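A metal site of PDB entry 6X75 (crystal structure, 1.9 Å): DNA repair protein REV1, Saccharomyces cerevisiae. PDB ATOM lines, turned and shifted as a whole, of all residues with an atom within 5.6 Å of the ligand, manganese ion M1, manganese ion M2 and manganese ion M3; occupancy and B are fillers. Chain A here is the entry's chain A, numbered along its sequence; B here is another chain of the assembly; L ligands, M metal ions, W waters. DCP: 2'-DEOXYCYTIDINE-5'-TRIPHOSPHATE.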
ATOM      1  N   ARG A  20     -18.843 -26.255  -7.555  1.00  0.00           N
ATOM      2  CA  ARG A  20     -18.801 -25.637  -6.247  1.00  0.00           C
ATOM      3  C   ARG A  20     -17.595 -26.096  -5.441  1.00  0.00           C
ATOM      4  O   ARG A  20     -17.038 -25.305  -4.669  1.00  0.00           O
ATOM      5  CB  ARG A  20     -20.102 -25.871  -5.477  1.00  0.00           C
ATOM      6  CG  ARG A  20     -20.059 -26.969  -4.425  1.00  0.00           C
ATOM      7  CD  ARG A  20     -20.460 -28.325  -4.988  1.00  0.00           C
ATOM      8  NE  ARG A  20     -20.620 -29.273  -3.885  1.00  0.00           N
ATOM      9  CZ  ARG A  20     -20.790 -30.590  -4.012  1.00  0.00           C
ATOM     10  NH1 ARG A  20     -20.833 -31.154  -5.205  1.00  0.00           N
ATOM     11  NH2 ARG A  20     -20.936 -31.350  -2.934  1.00  0.00           N
ATOM     12  N   LEU A  21     -17.131 -27.345  -5.655  1.00  0.00           N
ATOM     13  CA  LEU A  21     -15.955 -27.779  -4.891  1.00  0.00           C
ATOM     14  C   LEU A  21     -14.687 -27.076  -5.367  1.00  0.00           C
ATOM     15  O   LEU A  21     -13.806 -26.771  -4.548  1.00  0.00           O
ATOM     16  CB  LEU A  21     -15.785 -29.300  -4.951  1.00  0.00           C
ATOM     17  CG  LEU A  21     -16.933 -30.141  -4.359  1.00  0.00           C
ATOM     18  CD1 LEU A  21     -16.801 -31.633  -4.652  1.00  0.00           C
ATOM     19  CD2 LEU A  21     -17.044 -29.924  -2.867  1.00  0.00           C
ATOM     20  N   LEU A  24     -14.881 -23.729  -3.555  1.00  0.00           N
ATOM     21  CA  LEU A  24     -14.477 -23.857  -2.148  1.00  0.00           C
ATOM     22  C   LEU A  24     -12.960 -23.877  -2.004  1.00  0.00           C
ATOM     23  O   LEU A  24     -12.384 -23.178  -1.161  1.00  0.00           O
ATOM     24  CB  LEU A  24     -15.073 -25.125  -1.524  1.00  0.00           C
ATOM     25  CG  LEU A  24     -16.598 -25.168  -1.441  1.00  0.00           C
ATOM     26  CD1 LEU A  24     -17.080 -26.528  -0.963  1.00  0.00           C
ATOM     27  CD2 LEU A  24     -17.079 -24.079  -0.499  1.00  0.00           C
ATOM     28  N   ASP A  58     -18.980 -20.098  12.274  1.00  0.00           N
ATOM     29  CA  ASP A  58     -19.331 -20.764  11.013  1.00  0.00           C
ATOM     30  C   ASP A  58     -20.763 -20.407  10.601  1.00  0.00           C
ATOM     31  O   ASP A  58     -21.675 -20.480  11.429  1.00  0.00           O
ATOM     32  CB  ASP A  58     -19.165 -22.286  11.197  1.00  0.00           C
ATOM     33  CG  ASP A  58     -19.434 -23.051   9.930  1.00  0.00           C
ATOM     34  OD1 ASP A  58     -20.624 -23.276   9.612  1.00  0.00           O
ATOM     35  OD2 ASP A  58     -18.449 -23.455   9.282  1.00  0.00           O
ATOM     36  N   PHE A  59     -20.955 -20.056   9.329  1.00  0.00           N
ATOM     37  CA  PHE A  59     -22.304 -19.767   8.820  1.00  0.00           C
ATOM     38  C   PHE A  59     -23.218 -20.994   8.910  1.00  0.00           C
ATOM     39  O   PHE A  59     -22.821 -22.095   8.555  1.00  0.00           O
ATOM     40  CB  PHE A  59     -22.263 -19.374   7.341  1.00  0.00           C
ATOM     41  CG  PHE A  59     -21.824 -17.974   7.041  1.00  0.00           C
ATOM     42  CD1 PHE A  59     -20.484 -17.632   7.028  1.00  0.00           C
ATOM     43  CD2 PHE A  59     -22.753 -17.006   6.660  1.00  0.00           C
ATOM     44  CE1 PHE A  59     -20.073 -16.365   6.706  1.00  0.00           C
ATOM     45  CE2 PHE A  59     -22.351 -15.737   6.316  1.00  0.00           C
ATOM     46  CZ  PHE A  59     -21.006 -15.405   6.331  1.00  0.00           C
ATOM     47  N   ASP A  60     -24.467 -20.774   9.307  1.00  0.00           N
ATOM     48  CA  ASP A  60     -25.459 -21.836   9.218  1.00  0.00           C
ATOM     49  C   ASP A  60     -25.878 -22.031   7.771  1.00  0.00           C
ATOM     50  O   ASP A  60     -26.101 -21.055   7.039  1.00  0.00           O
ATOM     51  CB  ASP A  60     -26.676 -21.517  10.087  1.00  0.00           C
ATOM     52  CG  ASP A  60     -26.280 -21.099  11.498  1.00  0.00           C
ATOM     53  OD1 ASP A  60     -25.439 -21.811  12.109  1.00  0.00           O
ATOM     54  OD2 ASP A  60     -26.793 -20.081  11.988  1.00  0.00           O
ATOM     55  N   CYS A  61     -26.005 -23.300   7.363  1.00  0.00           N
ATOM     56  CA  CYS A  61     -26.232 -23.756   5.983  1.00  0.00           C
ATOM     57  C   CYS A  61     -25.927 -22.666   4.964  1.00  0.00           C
ATOM     58  O   CYS A  61     -26.833 -22.108   4.330  1.00  0.00           O
ATOM     59  CB  CYS A  61     -27.676 -24.266   5.810  1.00  0.00           C
ATOM     60  SG  CYS A  61     -28.933 -23.160   6.534  1.00  0.00           S
ATOM     61  N   PHE A  62     -24.635 -22.377   4.820  1.00  0.00           N
ATOM     62  CA  PHE A  62     -24.155 -21.162   4.148  1.00  0.00           C
ATOM     63  C   PHE A  62     -24.743 -20.972   2.755  1.00  0.00           C
ATOM     64  O   PHE A  62     -25.439 -19.986   2.495  1.00  0.00           O
ATOM     65  CB  PHE A  62     -22.641 -21.242   4.090  1.00  0.00           C
ATOM     66  CG  PHE A  62     -21.993 -20.061   3.415  1.00  0.00           C
ATOM     67  CD1 PHE A  62     -22.246 -18.788   3.837  1.00  0.00           C
ATOM     68  CD2 PHE A  62     -21.078 -20.252   2.376  1.00  0.00           C
ATOM     69  CE1 PHE A  62     -21.630 -17.709   3.258  1.00  0.00           C
ATOM     70  CE2 PHE A  62     -20.451 -19.193   1.778  1.00  0.00           C
ATOM     71  CZ  PHE A  62     -20.732 -17.913   2.208  1.00  0.00           C
ATOM     72  N   PHE A  63     -24.451 -21.907   1.822  1.00  0.00           N
ATOM     73  CA  PHE A  63     -24.980 -21.763   0.463  1.00  0.00           C
ATOM     74  C   PHE A  63     -26.509 -21.616   0.476  1.00  0.00           C
ATOM     75  O   PHE A  63     -27.061 -20.791  -0.257  1.00  0.00           O
ATOM     76  CB  PHE A  63     -24.602 -22.960  -0.404  1.00  0.00           C
ATOM     77  CG  PHE A  63     -23.165 -22.963  -0.905  1.00  0.00           C
ATOM     78  CD1 PHE A  63     -22.202 -22.090  -0.385  1.00  0.00           C
ATOM     79  CD2 PHE A  63     -22.782 -23.856  -1.901  1.00  0.00           C
ATOM     80  CE1 PHE A  63     -20.891 -22.118  -0.860  1.00  0.00           C
ATOM     81  CE2 PHE A  63     -21.480 -23.898  -2.383  1.00  0.00           C
ATOM     82  CZ  PHE A  63     -20.532 -23.040  -1.858  1.00  0.00           C
ATOM     83  N   ALA A  64     -27.187 -22.425   1.285  1.00  0.00           N
ATOM     84  CA  ALA A  64     -28.658 -22.376   1.293  1.00  0.00           C
ATOM     85  C   ALA A  64     -29.155 -21.008   1.751  1.00  0.00           C
ATOM     86  O   ALA A  64     -30.029 -20.407   1.125  1.00  0.00           O
ATOM     87  CB  ALA A  64     -29.217 -23.477   2.187  1.00  0.00           C
ATOM     88  N   ILE A  96     -26.418 -32.303  -3.362  1.00  0.00           N
ATOM     89  CA  ILE A  96     -26.941 -31.208  -2.556  1.00  0.00           C
ATOM     90  C   ILE A  96     -25.737 -30.554  -1.891  1.00  0.00           C
ATOM     91  O   ILE A  96     -25.080 -31.155  -1.043  1.00  0.00           O
ATOM     92  CB  ILE A  96     -27.965 -31.700  -1.519  1.00  0.00           C
ATOM     93  CG1 ILE A  96     -29.283 -32.032  -2.220  1.00  0.00           C
ATOM     94  CG2 ILE A  96     -28.154 -30.667  -0.407  1.00  0.00           C
ATOM     95  CD1 ILE A  96     -30.148 -32.958  -1.391  1.00  0.00           C
ATOM     96  N   ALA A  97     -25.408 -29.340  -2.331  1.00  0.00           N
ATOM     97  CA  ALA A  97     -24.249 -28.663  -1.761  1.00  0.00           C
ATOM     98  C   ALA A  97     -24.539 -28.220  -0.340  1.00  0.00           C
ATOM     99  O   ALA A  97     -23.693 -28.376   0.548  1.00  0.00           O
ATOM    100  CB  ALA A  97     -23.854 -27.479  -2.636  1.00  0.00           C
ATOM    101  N   SER A  98     -25.729 -27.678  -0.118  1.00  0.00           N
ATOM    102  CA  SER A  98     -26.133 -27.220   1.204  1.00  0.00           C
ATOM    103  C   SER A  98     -27.640 -27.379   1.304  1.00  0.00           C
ATOM    104  O   SER A  98     -28.376 -27.241   0.317  1.00  0.00           O
ATOM    105  CB  SER A  98     -25.691 -25.769   1.437  1.00  0.00           C
ATOM    106  OG  SER A  98     -26.135 -25.284   2.694  1.00  0.00           O
ATOM    107  N   CYS A  99     -28.105 -27.696   2.487  1.00  0.00           N
ATOM    108  CA  CYS A  99     -29.525 -27.769   2.737  1.00  0.00           C
ATOM    109  C   CYS A  99     -29.845 -27.104   4.058  1.00  0.00           C
ATOM    110  O   CYS A  99     -29.027 -27.100   4.985  1.00  0.00           O
ATOM    111  CB  CYS A  99     -29.992 -29.222   2.690  1.00  0.00           C
ATOM    112  SG  CYS A  99     -29.249 -30.222   4.015  1.00  0.00           S
ATOM    113  N   TYR A 101     -32.188 -26.153   7.557  1.00  0.00           N
ATOM    114  CA  TYR A 101     -32.441 -27.013   8.700  1.00  0.00           C
ATOM    115  C   TYR A 101     -33.827 -27.654   8.647  1.00  0.00           C
ATOM    116  O   TYR A 101     -33.998 -28.736   9.203  1.00  0.00           O
ATOM    117  CB  TYR A 101     -32.197 -26.208   9.990  1.00  0.00           C
ATOM    118  CG  TYR A 101     -30.714 -26.243  10.296  1.00  0.00           C
ATOM    119  CD1 TYR A 101     -29.812 -25.427   9.583  1.00  0.00           C
ATOM    120  CD2 TYR A 101     -30.183 -27.149  11.220  1.00  0.00           C
ATOM    121  CE1 TYR A 101     -28.434 -25.478   9.829  1.00  0.00           C
ATOM    122  CE2 TYR A 101     -28.808 -27.208  11.470  1.00  0.00           C
ATOM    123  CZ  TYR A 101     -27.946 -26.379  10.766  1.00  0.00           C
ATOM    124  OH  TYR A 101     -26.589 -26.423  11.007  1.00  0.00           O
ATOM    125  N   ARG A 104     -33.036 -30.735   6.912  1.00  0.00           N
ATOM    126  CA  ARG A 104     -32.299 -31.668   7.755  1.00  0.00           C
ATOM    127  C   ARG A 104     -33.208 -32.370   8.763  1.00  0.00           C
ATOM    128  O   ARG A 104     -32.888 -33.488   9.205  1.00  0.00           O
ATOM    129  CB  ARG A 104     -31.175 -30.934   8.477  1.00  0.00           C
ATOM    130  CG  ARG A 104     -30.195 -30.257   7.505  1.00  0.00           C
ATOM    131  CD  ARG A 104     -28.990 -29.648   8.201  1.00  0.00           C
ATOM    132  NE  ARG A 104     -28.235 -28.826   7.256  1.00  0.00           N
ATOM    133  CZ  ARG A 104     -27.002 -28.363   7.455  1.00  0.00           C
ATOM    134  NH1 ARG A 104     -26.353 -28.648   8.583  1.00  0.00           N
ATOM    135  NH2 ARG A 104     -26.422 -27.618   6.499  1.00  0.00           N
ATOM    136  N   ASN A 110     -25.919 -32.470   3.625  1.00  0.00           N
ATOM    137  CA  ASN A 110     -25.064 -31.984   2.553  1.00  0.00           C
ATOM    138  C   ASN A 110     -24.384 -33.168   1.884  1.00  0.00           C
ATOM    139  O   ASN A 110     -23.952 -34.109   2.553  1.00  0.00           O
ATOM    140  CB  ASN A 110     -23.990 -31.034   3.093  1.00  0.00           C
ATOM    141  CG  ASN A 110     -24.574 -29.728   3.607  1.00  0.00           C
ATOM    142  OD1 ASN A 110     -25.744 -29.432   3.411  1.00  0.00           O
ATOM    143  ND2 ASN A 110     -23.728 -28.924   4.247  1.00  0.00           N
ATOM    144  N   GLY A 111     -24.270 -33.116   0.556  1.00  0.00           N
ATOM    145  CA  GLY A 111     -23.586 -34.153  -0.180  1.00  0.00           C
ATOM    146  C   GLY A 111     -24.481 -35.270  -0.662  1.00  0.00           C
ATOM    147  O   GLY A 111     -24.039 -36.071  -1.500  1.00  0.00           O
ATOM    148  N   SER A 161     -12.413 -21.606   5.959  1.00  0.00           N
ATOM    149  CA  SER A 161     -13.055 -21.775   4.674  1.00  0.00           C
ATOM    150  C   SER A 161     -13.749 -20.480   4.309  1.00  0.00           C
ATOM    151  O   SER A 161     -13.650 -19.467   5.031  1.00  0.00           O
ATOM    152  CB  SER A 161     -14.053 -22.941   4.714  1.00  0.00           C
ATOM    153  OG  SER A 161     -15.272 -22.556   5.335  1.00  0.00           O
ATOM    154  N   ILE A 162     -14.432 -20.513   3.171  1.00  0.00           N
ATOM    155  CA  ILE A 162     -15.330 -19.430   2.771  1.00  0.00           C
ATOM    156  C   ILE A 162     -16.306 -19.054   3.880  1.00  0.00           C
ATOM    157  O   ILE A 162     -16.699 -17.881   3.997  1.00  0.00           O
ATOM    158  CB  ILE A 162     -16.073 -19.832   1.473  1.00  0.00           C
ATOM    159  CG1 ILE A 162     -16.831 -18.633   0.904  1.00  0.00           C
ATOM    160  CG2 ILE A 162     -17.060 -20.995   1.716  1.00  0.00           C
ATOM    161  CD1 ILE A 162     -15.907 -17.576   0.271  1.00  0.00           C
ATOM    162  N   ASP A 163     -16.754 -20.006   4.709  1.00  0.00           N
ATOM    163  CA  ASP A 163     -17.816 -19.701   5.653  1.00  0.00           C
ATOM    164  C   ASP A 163     -17.386 -19.890   7.105  1.00  0.00           C
ATOM    165  O   ASP A 163     -18.231 -20.039   7.987  1.00  0.00           O
ATOM    166  CB  ASP A 163     -19.088 -20.502   5.337  1.00  0.00           C
ATOM    167  CG  ASP A 163     -19.136 -21.853   6.049  1.00  0.00           C
ATOM    168  OD1 ASP A 163     -18.115 -22.579   6.124  1.00  0.00           O
ATOM    169  OD2 ASP A 163     -20.225 -22.178   6.594  1.00  0.00           O
ATOM    170  N   GLU A 164     -16.089 -19.874   7.388  1.00  0.00           N
ATOM    171  CA  GLU A 164     -15.681 -20.396   8.682  1.00  0.00           C
ATOM    172  C   GLU A 164     -14.328 -19.850   9.071  1.00  0.00           C
ATOM    173  O   GLU A 164     -13.402 -19.870   8.251  1.00  0.00           O
ATOM    174  CB  GLU A 164     -15.639 -21.922   8.598  1.00  0.00           C
ATOM    175  CG  GLU A 164     -15.212 -22.632   9.845  1.00  0.00           C
ATOM    176  CD  GLU A 164     -15.393 -24.123   9.686  1.00  0.00           C
ATOM    177  OE1 GLU A 164     -14.954 -24.871  10.581  1.00  0.00           O
ATOM    178  OE2 GLU A 164     -15.967 -24.541   8.642  1.00  0.00           O
ATOM    179  N   ARG A 214     -14.685 -26.722  18.256  1.00  0.00           N
ATOM    180  CA  ARG A 214     -15.335 -27.358  17.108  1.00  0.00           C
ATOM    181  C   ARG A 214     -16.559 -28.150  17.545  1.00  0.00           C
ATOM    182  O   ARG A 214     -17.620 -28.082  16.906  1.00  0.00           O
ATOM    183  CB  ARG A 214     -14.346 -28.258  16.373  1.00  0.00           C
ATOM    184  CG  ARG A 214     -14.959 -28.996  15.179  1.00  0.00           C
ATOM    185  CD  ARG A 214     -15.348 -28.021  14.059  1.00  0.00           C
ATOM    186  NE  ARG A 214     -16.101 -28.663  12.978  1.00  0.00           N
ATOM    187  CZ  ARG A 214     -17.425 -28.766  12.949  1.00  0.00           C
ATOM    188  NH1 ARG A 214     -18.148 -28.274  13.955  1.00  0.00           N
ATOM    189  NH2 ARG A 214     -18.025 -29.364  11.930  1.00  0.00           N
ATOM    190  N   LYS A 221     -25.266 -25.207  16.825  1.00  0.00           N
ATOM    191  CA  LYS A 221     -26.052 -25.020  15.607  1.00  0.00           C
ATOM    192  C   LYS A 221     -27.475 -25.548  15.786  1.00  0.00           C
ATOM    193  O   LYS A 221     -27.698 -26.518  16.505  1.00  0.00           O
ATOM    194  CB  LYS A 221     -25.386 -25.732  14.432  1.00  0.00           C
ATOM    195  CG  LYS A 221     -24.369 -24.876  13.747  1.00  0.00           C
ATOM    196  CD  LYS A 221     -23.550 -25.645  12.735  1.00  0.00           C
ATOM    197  CE  LYS A 221     -22.489 -24.725  12.136  1.00  0.00           C
ATOM    198  NZ  LYS A 221     -23.105 -23.581  11.400  1.00  0.00           N
ATOM    199  P    DG B  12     -13.140 -29.534   9.416  1.00  0.00           P
ATOM    200  OP1  DG B  12     -13.502 -28.881  10.708  1.00  0.00           O
ATOM    201  OP2  DG B  12     -14.026 -30.566   8.855  1.00  0.00           O
ATOM    202  O5'  DG B  12     -12.947 -28.351   8.375  1.00  0.00           O
ATOM    203  C5'  DG B  12     -13.624 -28.392   7.172  1.00  0.00           C
ATOM    204  C4'  DG B  12     -13.062 -27.365   6.230  1.00  0.00           C
ATOM    205  O4'  DG B  12     -11.760 -27.827   5.768  1.00  0.00           O
ATOM    206  C3'  DG B  12     -13.891 -27.188   4.966  1.00  0.00           C
ATOM    207  O3'  DG B  12     -14.853 -26.149   5.122  1.00  0.00           O
ATOM    208  C2'  DG B  12     -12.812 -26.819   3.945  1.00  0.00           C
ATOM    209  C1'  DG B  12     -11.722 -27.796   4.354  1.00  0.00           C
ATOM    210  N9   DG B  12     -11.971 -29.148   3.832  1.00  0.00           N
ATOM    211  C8   DG B  12     -12.378 -30.279   4.526  1.00  0.00           C
ATOM    212  N7   DG B  12     -12.553 -31.316   3.753  1.00  0.00           N
ATOM    213  C5   DG B  12     -12.248 -30.849   2.479  1.00  0.00           C
ATOM    214  C6   DG B  12     -12.248 -31.513   1.211  1.00  0.00           C
ATOM    215  O6   DG B  12     -12.530 -32.705   0.955  1.00  0.00           O
ATOM    216  N1   DG B  12     -11.876 -30.649   0.180  1.00  0.00           N
ATOM    217  C2   DG B  12     -11.538 -29.313   0.343  1.00  0.00           C
ATOM    218  N2   DG B  12     -11.192 -28.642  -0.757  1.00  0.00           N
ATOM    219  N3   DG B  12     -11.529 -28.703   1.501  1.00  0.00           N
ATOM    220  C4   DG B  12     -11.898 -29.516   2.513  1.00  0.00           C
ATOM    221  P    DC B  13     -16.380 -26.479   5.531  1.00  0.00           P
ATOM    222  OP1  DC B  13     -17.160 -25.215   5.497  1.00  0.00           O
ATOM    223  OP2  DC B  13     -16.315 -27.242   6.799  1.00  0.00           O
ATOM    224  O5'  DC B  13     -16.931 -27.479   4.421  1.00  0.00           O
ATOM    225  C5'  DC B  13     -16.772 -27.195   3.043  1.00  0.00           C
ATOM    226  C4'  DC B  13     -16.160 -28.389   2.313  1.00  0.00           C
ATOM    227  O4'  DC B  13     -15.497 -29.268   3.257  1.00  0.00           O
ATOM    228  C3'  DC B  13     -17.141 -29.267   1.543  1.00  0.00           C
ATOM    229  O3'  DC B  13     -16.631 -29.528   0.241  1.00  0.00           O
ATOM    230  C2'  DC B  13     -17.197 -30.552   2.384  1.00  0.00           C
ATOM    231  C1'  DC B  13     -15.781 -30.593   2.902  1.00  0.00           C
ATOM    232  N1   DC B  13     -15.583 -31.468   4.084  1.00  0.00           N
ATOM    233  C2   DC B  13     -15.488 -32.858   3.912  1.00  0.00           C
ATOM    234  O2   DC B  13     -15.611 -33.343   2.775  1.00  0.00           O
ATOM    235  N3   DC B  13     -15.274 -33.646   5.003  1.00  0.00           N
ATOM    236  C4   DC B  13     -15.144 -33.090   6.210  1.00  0.00           C
ATOM    237  N4   DC B  13     -14.948 -33.902   7.253  1.00  0.00           N
ATOM    238  C5   DC B  13     -15.230 -31.674   6.408  1.00  0.00           C
ATOM    239  C6   DC B  13     -15.440 -30.907   5.326  1.00  0.00           C
HETATM  240  N1  DCP L   1     -20.523 -27.726   0.907  1.00  0.00           N
HETATM  241  C2  DCP L   1     -20.603 -28.520  -0.341  1.00  0.00           C
HETATM  242  N3  DCP L   1     -20.641 -29.996  -0.279  1.00  0.00           N
HETATM  243  C4  DCP L   1     -20.610 -30.660   0.993  1.00  0.00           C
HETATM  244  C5  DCP L   1     -20.533 -29.861   2.265  1.00  0.00           C
HETATM  245  C6  DCP L   1     -20.478 -28.385   2.196  1.00  0.00           C
HETATM  246  O2  DCP L   1     -20.641 -27.935  -1.371  1.00  0.00           O
HETATM  247  N4  DCP L   1     -20.637 -32.098   1.024  1.00  0.00           N
HETATM  248  C1' DCP L   1     -20.504 -26.296   0.724  1.00  0.00           C
HETATM  249  C2' DCP L   1     -21.752 -25.834   0.883  1.00  0.00           C
HETATM  250  C3' DCP L   1     -21.799 -25.308   2.413  1.00  0.00           C
HETATM  251  C4' DCP L   1     -20.582 -24.673   2.525  1.00  0.00           C
HETATM  252  O4' DCP L   1     -19.635 -25.643   1.849  1.00  0.00           O
HETATM  253  O3' DCP L   1     -22.919 -24.434   2.576  1.00  0.00           O
HETATM  254  C5' DCP L   1     -20.053 -24.610   3.938  1.00  0.00           C
HETATM  255  O5' DCP L   1     -19.855 -25.940   4.365  1.00  0.00           O
HETATM  256  PA  DCP L   1     -20.310 -26.297   5.898  1.00  0.00           P
HETATM  257  O1A DCP L   1     -19.955 -25.125   6.829  1.00  0.00           O
HETATM  258  O2A DCP L   1     -19.675 -27.606   6.334  1.00  0.00           O
HETATM  259  O3A DCP L   1     -21.971 -26.610   5.891  1.00  0.00           O
HETATM  260  PB  DCP L   1     -23.206 -25.562   5.860  1.00  0.00           P
HETATM  261  O1B DCP L   1     -24.068 -25.748   4.599  1.00  0.00           O
HETATM  262  O2B DCP L   1     -22.683 -24.124   6.077  1.00  0.00           O
HETATM  263  O3B DCP L   1     -24.219 -26.009   7.104  1.00  0.00           O
HETATM  264  PG  DCP L   1     -23.793 -25.984   8.709  1.00  0.00           P
HETATM  265  O1G DCP L   1     -24.788 -25.032   9.420  1.00  0.00           O
HETATM  266  O2G DCP L   1     -23.901 -27.411   9.231  1.00  0.00           O
HETATM  267  O3G DCP L   1     -22.386 -25.479   8.848  1.00  0.00           O
HETATM  268 MN    MN M   1     -18.001 -24.505   7.456  1.00  0.00          MN
HETATM  269 MN    MN M   2     -18.347 -28.589   7.441  1.00  0.00          MN
HETATM  270 MN    MN M   3     -21.458 -23.675   7.738  1.00  0.00          MN
HETATM  271  O   HOH W   1     -16.596 -29.832   8.920  1.00  0.00           O
HETATM  272  O   HOH W   2     -23.135 -28.805  11.296  1.00  0.00           O
HETATM  273  O   HOH W   3     -19.913 -33.688  -1.401  1.00  0.00           O
HETATM  274  O   HOH W   4     -18.904 -30.436   5.882  1.00  0.00           O
HETATM  275  O   HOH W   5     -20.142 -33.463   3.526  1.00  0.00           O
HETATM  276  O   HOH W   6     -20.085 -29.251   9.139  1.00  0.00           O
HETATM  277  O   HOH W   7     -17.902 -26.456   8.590  1.00  0.00           O
HETATM  278  O   HOH W   8     -21.508 -29.994   5.498  1.00  0.00           O
HETATM  279  O   HOH W   9     -20.283 -26.737   9.895  1.00  0.00           O
HETATM  280  O   HOH W  10     -22.932 -29.632   7.958  1.00  0.00           O
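The side-chain hydroxyl (OH) of Tyr 101 is in hydrogen-bond range of an oxygen (O1G) of the ligand (2.8 Å).
NH1 of Arg 104 is in salt-bridge range of O2G of the ligand, 2.8 Å away.
An oxygen (O2) of the ligand sits at hydrogen-bond distance from the guanidinium group (NE) of Arg 20, at 2.8 Å.
An oxygen (O1B) of the ligand is in hydrogen-bond range of the side-chain hydroxyl (OG) of Ser 98, 2.8 Å away.
O1B of the ligand sits at hydrogen-bond distance from N of Phe 62, 3.4 Å away.
The backbone NH (N) of Cys 61 is in hydrogen-bond range of an oxygen (O1G) of the ligand (3.0 Å).
The side-chain amino group (NZ) of Lys 221 is in salt-bridge range of an oxygen (O1G) of the ligand, at 3.0 Å.
O3' of the ligand is in hydrogen-bond range of N of Phe 63, at 3.0 Å.
O1B of the ligand sits at hydrogen-bond distance from ND2 of Asn 110 (3.2 Å).
The side-chain amino group of Lys 221 lies within hydrogen-bond range of the backbone carbonyl oxygen of Asp 58, 3.4 Å away.
The backbone carbonyl oxygen (O) of Phe 59 sits close to the side-chain amino group (NZ) of Lys 221 (3.2 Å).
OP1 of DC 13 of chain B sits close to the side-chain hydroxyl (OG) of Ser 161, 3.3 Å away.
N of Glu 164 lies close to OG of Ser 161 (3.5 Å).
The backbone carbonyl oxygen (O) of Cys 99 is in hydrogen-bond range of the guanidinium group (NE) of Arg 104, at 3.0 Å.
The side-chain hydroxyl (OG) of Ser 98 sits at hydrogen-bond distance from the backbone NH (N) of Ala 64.
NZ of Lys 221 lies within salt-bridge range of OD1 of Asp 60 (3.0 Å).
The backbone carbonyl oxygen (O) of Ile 96 sits at hydrogen-bond distance from the backbone NH (N) of Gly 111 (2.7 Å).
A nitrogen (N1) of the ligand lies close to the backbone carbonyl oxygen (O) of Ala 97, at 3.3 Å.
Leu 24 touches the ligand (CD2 to O4', 3.8 Å).
CA of Asp 60 touches O1G of the ligand (3.3 Å).
Gly 111 touches the ligand (CA to N4, 3.8 Å).
Of the 26 residues printed, 17 come within 4 Å of the ligand.
Along chain A the residues within 4 Å of the ligand span positions 20 to 221.
Residues that only touch manganese ion M1: Ser 161 (3.97 Å).
Five residues have an atom within 4 Å of manganese ion M1: Asp 58, Ser 161, Asp 163, Glu 164 and DC 13 of chain B.
The nearest printed residue that does not touch manganese ion M1 is DG 12 of chain B (4.2 Å).
Within 4 Å of manganese ion M2: DC 13 of chain B.
The nearest printed residue that does not touch manganese ion M2 is Arg 214 (4.6 Å).
Of the 26 residues printed, 3 come within 4 Å of manganese ion M3.
The nearest printed residue that does not touch manganese ion M3 is Lys 221 (4.02 Å).
Manganese ion M1 is bound by an oxygen (O1A) of the ligand (2.1 Å), the side-chain carboxylate of Asp 58 (2.2 Å), OP1 of DC 13 of chain B (2.2 Å), water W7 (2.3 Å), the side-chain carboxylate of Asp 163 (2.3 Å) and the side-chain carboxylate of Glu 164 (2.4 Å).
Manganese ion M2 is bound by an oxygen (O2A) of the ligand (2.0 Å), water W7 (2.5 Å), water W4 (2.5 Å), water W6 (2.5 Å), OP2 of DC 13 of chain B (2.5 Å) and water W1 (2.6 Å).
Manganese ion M2 has six donor atoms within binding distance.
Manganese ion M3 is bound by OD1 of Asp 58 (2.1 Å), O2B of the ligand (2.1 Å), O of Phe 59 (2.2 Å), OD2 of Asp 163 (2.3 Å), O1A of the ligand (2.3 Å) and O3G of the ligand (2.3 Å).
Water W1 lies within hydrogen-bond range of OP2 of DG 12 of chain B (2.7 Å) and the guanidinium group of Arg 214 (3.4 Å).
Water W3 bridges NH2 of Arg 20 and N4 of the ligand.
Water W8 lies within hydrogen-bond range of the side-chain amide nitrogen (ND2) of Asn 110 and an oxygen (O3A) of the ligand.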
